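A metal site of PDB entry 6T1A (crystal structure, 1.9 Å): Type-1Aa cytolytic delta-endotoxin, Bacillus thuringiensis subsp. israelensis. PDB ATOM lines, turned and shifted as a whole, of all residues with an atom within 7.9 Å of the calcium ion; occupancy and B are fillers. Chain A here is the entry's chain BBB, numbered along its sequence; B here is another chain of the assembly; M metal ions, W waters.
OE1 of Glu 32 of chain B is bound to the calcium ion, at 2.2 Å.
The calcium ion is bound by the backbone carbonyl oxygen (O) of Ser 134 (2.2 Å).
Water W3 binds the calcium ion (2.3 Å).
Water W4 is bound to the calcium ion, 2.5 Å away.
The calcium ion is bound by water W2, at 2.6 Å.
The calcium ion is bound by OE2 of Glu 45 (2.6 Å).
The calcium ion is bound by water W1, 2.9 Å away.
Water W3 lies within hydrogen-bond range of OE1 of Gln 138 (2.5 Å), NE of Arg 30 of chain B (2.9 Å) and OE1 of Glu 45 (3.0 Å).
The side-chain carboxylate (OE1) of Glu 32 of chain B lies close to the guanidinium group (NE) of Arg 30 of chain B (3.1 Å).
O of Ile 46 sits at hydrogen-bond distance from N of Glu 32 of chain B (3.0 Å).
OG of Ser 134 sits at hydrogen-bond distance from ND2 of Asn 181 (3.2 Å).
The side-chain hydroxyl (OG) of Ser 134 sits at hydrogen-bond distance from the backbone carbonyl oxygen (O) of Leu 131.
OE1 of Glu 45 sits at hydrogen-bond distance from NE2 of Gln 138 (2.4 Å).
The side-chain amide nitrogen of Asn 181 sits close to the side-chain carboxylate of Glu 45 (3.3 Å).
The backbone NH of Gln 180 is in hydrogen-bond range of the backbone carbonyl oxygen of Glu 45 (2.9 Å).
The nearest printed residue that does not touch the calcium ion is Val 135 (4.3 Å).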
ATOM      1  N   SER A  22      -5.656 -39.518  31.786  1.00  0.00           N
ATOM      2  CA  SER A  22      -4.888 -38.616  30.933  1.00  0.00           C
ATOM      3  C   SER A  22      -3.728 -39.361  30.291  1.00  0.00           C
ATOM      4  O   SER A  22      -3.211 -40.328  30.852  1.00  0.00           O
ATOM      5  CB  SER A  22      -4.405 -37.417  31.720  1.00  0.00           C
ATOM      6  OG  SER A  22      -3.631 -36.558  30.894  1.00  0.00           O
ATOM      7  N   ALA A  24      -1.293 -37.280  29.155  1.00  0.00           N
ATOM      8  CA  ALA A  24      -0.374 -36.149  29.215  1.00  0.00           C
ATOM      9  C   ALA A  24       0.903 -36.533  29.951  1.00  0.00           C
ATOM     10  O   ALA A  24       0.855 -37.178  30.993  1.00  0.00           O
ATOM     11  CB  ALA A  24      -1.037 -34.961  29.856  1.00  0.00           C
ATOM     12  N   GLU A  45       1.697 -25.440  29.966  1.00  0.00           N
ATOM     13  CA  GLU A  45       0.816 -26.309  29.219  1.00  0.00           C
ATOM     14  C   GLU A  45       1.157 -26.161  27.743  1.00  0.00           C
ATOM     15  O   GLU A  45       1.084 -25.067  27.193  1.00  0.00           O
ATOM     16  CB  GLU A  45      -0.640 -25.906  29.454  1.00  0.00           C
ATOM     17  CG  GLU A  45      -1.602 -26.418  28.403  1.00  0.00           C
ATOM     18  CD  GLU A  45      -2.453 -27.604  28.828  1.00  0.00           C
ATOM     19  OE1 GLU A  45      -2.293 -28.077  29.969  1.00  0.00           O
ATOM     20  OE2 GLU A  45      -3.302 -28.039  28.016  1.00  0.00           O
ATOM     21  N   ILE A  46       1.527 -27.280  27.098  1.00  0.00           N
ATOM     22  CA  ILE A  46       2.033 -27.258  25.745  1.00  0.00           C
ATOM     23  C   ILE A  46       1.677 -28.584  25.079  1.00  0.00           C
ATOM     24  O   ILE A  46       1.922 -29.641  25.655  1.00  0.00           O
ATOM     25  CB  ILE A  46       3.547 -27.003  25.744  1.00  0.00           C
ATOM     26  CG1 ILE A  46       3.886 -25.560  25.356  1.00  0.00           C
ATOM     27  CG2 ILE A  46       4.275 -28.002  24.858  1.00  0.00           C
ATOM     28  CD1 ILE A  46       3.560 -24.544  26.432  1.00  0.00           C
ATOM     29  N   LEU A 131     -10.388 -21.534  27.966  1.00  0.00           N
ATOM     30  CA  LEU A 131      -9.006 -21.632  28.411  1.00  0.00           C
ATOM     31  C   LEU A 131      -8.943 -22.312  29.778  1.00  0.00           C
ATOM     32  O   LEU A 131      -8.128 -23.211  29.988  1.00  0.00           O
ATOM     33  CB  LEU A 131      -8.390 -20.234  28.437  1.00  0.00           C
ATOM     34  CG  LEU A 131      -6.882 -20.146  28.209  1.00  0.00           C
ATOM     35  CD1 LEU A 131      -6.462 -20.905  26.962  1.00  0.00           C
ATOM     36  CD2 LEU A 131      -6.433 -18.699  28.111  1.00  0.00           C
ATOM     37  N   SER A 132      -9.829 -21.899  30.704  1.00  0.00           N
ATOM     38  CA  SER A 132      -9.947 -22.482  32.022  1.00  0.00           C
ATOM     39  C   SER A 132     -10.016 -24.011  31.948  1.00  0.00           C
ATOM     40  O   SER A 132      -9.232 -24.700  32.601  1.00  0.00           O
ATOM     41  CB  SER A 132     -11.146 -21.931  32.764  1.00  0.00           C
ATOM     42  OG  SER A 132     -10.915 -20.595  33.191  1.00  0.00           O
ATOM     43  N   GLY A 133     -10.965 -24.505  31.140  1.00  0.00           N
ATOM     44  CA  GLY A 133     -11.255 -25.926  31.034  1.00  0.00           C
ATOM     45  C   GLY A 133     -10.068 -26.738  30.507  1.00  0.00           C
ATOM     46  O   GLY A 133      -9.934 -27.919  30.843  1.00  0.00           O
ATOM     47  N   SER A 134      -9.214 -26.102  29.713  1.00  0.00           N
ATOM     48  CA  SER A 134      -8.089 -26.768  29.070  1.00  0.00           C
ATOM     49  C   SER A 134      -6.900 -26.921  30.018  1.00  0.00           C
ATOM     50  O   SER A 134      -5.922 -27.584  29.659  1.00  0.00           O
ATOM     51  CB  SER A 134      -7.701 -26.054  27.797  1.00  0.00           C
ATOM     52  OG  SER A 134      -7.260 -24.736  28.072  1.00  0.00           O
ATOM     53  N   VAL A 135      -6.978 -26.307  31.209  1.00  0.00           N
ATOM     54  CA  VAL A 135      -5.873 -26.300  32.156  1.00  0.00           C
ATOM     55  C   VAL A 135      -6.394 -26.415  33.589  1.00  0.00           C
ATOM     56  O   VAL A 135      -5.730 -25.950  34.512  1.00  0.00           O
ATOM     57  CB  VAL A 135      -4.968 -25.063  31.976  1.00  0.00           C
ATOM     58  CG1 VAL A 135      -4.350 -24.972  30.595  1.00  0.00           C
ATOM     59  CG2 VAL A 135      -5.687 -23.769  32.329  1.00  0.00           C
ATOM     60  N   ILE A 136      -7.564 -27.045  33.772  1.00  0.00           N
ATOM     61  CA  ILE A 136      -8.269 -27.041  35.042  1.00  0.00           C
ATOM     62  C   ILE A 136      -7.496 -27.800  36.120  1.00  0.00           C
ATOM     63  O   ILE A 136      -7.551 -27.432  37.292  1.00  0.00           O
ATOM     64  CB  ILE A 136      -9.719 -27.552  34.894  1.00  0.00           C
ATOM     65  CG1 ILE A 136     -10.600 -27.170  36.096  1.00  0.00           C
ATOM     66  CG2 ILE A 136      -9.757 -29.048  34.617  1.00  0.00           C
ATOM     67  CD1 ILE A 136     -10.803 -25.687  36.276  1.00  0.00           C
ATOM     68  N   ASP A 137      -6.785 -28.852  35.714  1.00  0.00           N
ATOM     69  CA  ASP A 137      -6.070 -29.729  36.636  1.00  0.00           C
ATOM     70  C   ASP A 137      -4.900 -28.995  37.276  1.00  0.00           C
ATOM     71  O   ASP A 137      -4.759 -28.991  38.498  1.00  0.00           O
ATOM     72  CB  ASP A 137      -5.624 -31.023  35.937  1.00  0.00           C
ATOM     73  CG  ASP A 137      -6.767 -31.923  35.508  1.00  0.00           C
ATOM     74  OD1 ASP A 137      -7.870 -31.791  36.089  1.00  0.00           O
ATOM     75  OD2 ASP A 137      -6.560 -32.750  34.598  1.00  0.00           O
ATOM     76  N   GLN A 138      -4.052 -28.368  36.440  1.00  0.00           N
ATOM     77  CA  GLN A 138      -2.867 -27.675  36.930  1.00  0.00           C
ATOM     78  C   GLN A 138      -3.262 -26.365  37.621  1.00  0.00           C
ATOM     79  O   GLN A 138      -2.558 -25.920  38.531  1.00  0.00           O
ATOM     80  CB  GLN A 138      -1.841 -27.448  35.823  1.00  0.00           C
ATOM     81  CG  GLN A 138      -2.377 -26.728  34.600  1.00  0.00           C
ATOM     82  CD  GLN A 138      -2.685 -27.671  33.470  1.00  0.00           C
ATOM     83  OE1 GLN A 138      -3.395 -28.661  33.627  1.00  0.00           O
ATOM     84  NE2 GLN A 138      -2.137 -27.371  32.301  1.00  0.00           N
ATOM     85  N   ILE A 179       0.232 -21.213  28.311  1.00  0.00           N
ATOM     86  CA  ILE A 179      -0.768 -22.079  27.716  1.00  0.00           C
ATOM     87  C   ILE A 179      -0.647 -22.018  26.199  1.00  0.00           C
ATOM     88  O   ILE A 179      -0.765 -20.948  25.596  1.00  0.00           O
ATOM     89  CB  ILE A 179      -2.193 -21.704  28.191  1.00  0.00           C
ATOM     90  CG1 ILE A 179      -2.284 -21.556  29.705  1.00  0.00           C
ATOM     91  CG2 ILE A 179      -3.227 -22.684  27.656  1.00  0.00           C
ATOM     92  CD1 ILE A 179      -3.511 -20.807  30.189  1.00  0.00           C
ATOM     93  N   GLN A 180      -0.409 -23.192  25.586  1.00  0.00           N
ATOM     94  CA  GLN A 180      -0.429 -23.388  24.144  1.00  0.00           C
ATOM     95  C   GLN A 180      -1.103 -24.734  23.856  1.00  0.00           C
ATOM     96  O   GLN A 180      -0.539 -25.790  24.151  1.00  0.00           O
ATOM     97  CB  GLN A 180       0.996 -23.337  23.582  1.00  0.00           C
ATOM     98  CG  GLN A 180       1.080 -23.570  22.078  1.00  0.00           C
ATOM     99  CD  GLN A 180       1.049 -25.035  21.706  1.00  0.00           C
ATOM    100  OE1 GLN A 180       1.773 -25.866  22.270  1.00  0.00           O
ATOM    101  NE2 GLN A 180       0.208 -25.373  20.750  1.00  0.00           N
ATOM    102  N   ASN A 181      -2.304 -24.670  23.271  1.00  0.00           N
ATOM    103  CA  ASN A 181      -3.109 -25.847  22.994  1.00  0.00           C
ATOM    104  C   ASN A 181      -4.141 -25.507  21.922  1.00  0.00           C
ATOM    105  O   ASN A 181      -4.046 -24.475  21.264  1.00  0.00           O
ATOM    106  CB  ASN A 181      -3.731 -26.422  24.276  1.00  0.00           C
ATOM    107  CG  ASN A 181      -4.637 -25.450  24.998  1.00  0.00           C
ATOM    108  OD1 ASN A 181      -5.313 -24.631  24.368  1.00  0.00           O
ATOM    109  ND2 ASN A 181      -4.683 -25.537  26.310  1.00  0.00           N
ATOM    110  N   ARG B  30       3.703 -29.714  31.129  1.00  0.00           N
ATOM    111  CA  ARG B  30       2.629 -30.643  30.830  1.00  0.00           C
ATOM    112  C   ARG B  30       2.482 -30.736  29.311  1.00  0.00           C
ATOM    113  O   ARG B  30       2.049 -29.780  28.671  1.00  0.00           O
ATOM    114  CB  ARG B  30       1.317 -30.194  31.489  1.00  0.00           C
ATOM    115  CG  ARG B  30       0.189 -31.196  31.353  1.00  0.00           C
ATOM    116  CD  ARG B  30      -1.154 -30.692  31.871  1.00  0.00           C
ATOM    117  NE  ARG B  30      -2.194 -31.702  31.773  1.00  0.00           N
ATOM    118  CZ  ARG B  30      -2.337 -32.717  32.621  1.00  0.00           C
ATOM    119  NH1 ARG B  30      -3.325 -33.573  32.455  1.00  0.00           N
ATOM    120  NH2 ARG B  30      -1.492 -32.866  33.630  1.00  0.00           N
ATOM    121  N   VAL B  31       2.873 -31.888  28.759  1.00  0.00           N
ATOM    122  CA  VAL B  31       2.858 -32.115  27.323  1.00  0.00           C
ATOM    123  C   VAL B  31       1.623 -32.925  26.953  1.00  0.00           C
ATOM    124  O   VAL B  31       1.569 -34.140  27.177  1.00  0.00           O
ATOM    125  CB  VAL B  31       4.164 -32.790  26.838  1.00  0.00           C
ATOM    126  CG1 VAL B  31       4.191 -32.953  25.333  1.00  0.00           C
ATOM    127  CG2 VAL B  31       5.404 -32.030  27.312  1.00  0.00           C
ATOM    128  N   GLU B  32       0.626 -32.236  26.389  1.00  0.00           N
ATOM    129  CA  GLU B  32      -0.627 -32.842  25.978  1.00  0.00           C
ATOM    130  C   GLU B  32      -0.415 -33.645  24.690  1.00  0.00           C
ATOM    131  O   GLU B  32       0.348 -33.234  23.813  1.00  0.00           O
ATOM    132  CB  GLU B  32      -1.698 -31.775  25.743  1.00  0.00           C
ATOM    133  CG  GLU B  32      -2.074 -31.005  26.994  1.00  0.00           C
ATOM    134  CD  GLU B  32      -2.868 -31.757  28.057  1.00  0.00           C
ATOM    135  OE1 GLU B  32      -3.416 -31.089  28.948  1.00  0.00           O
ATOM    136  OE2 GLU B  32      -2.943 -32.997  27.979  1.00  0.00           O
HETATM  137 CA    CA M   1      -4.991 -29.579  29.310  1.00  0.00          CA
HETATM  138  O   HOH W   1      -5.914 -32.285  28.974  1.00  0.00           O
HETATM  139  O   HOH W   2      -7.335 -30.360  30.150  1.00  0.00           O
HETATM  140  O   HOH W   3      -4.326 -29.686  31.518  1.00  0.00           O
HETATM  141  O   HOH W   4      -5.317 -29.899  26.881  1.00  0.00           O
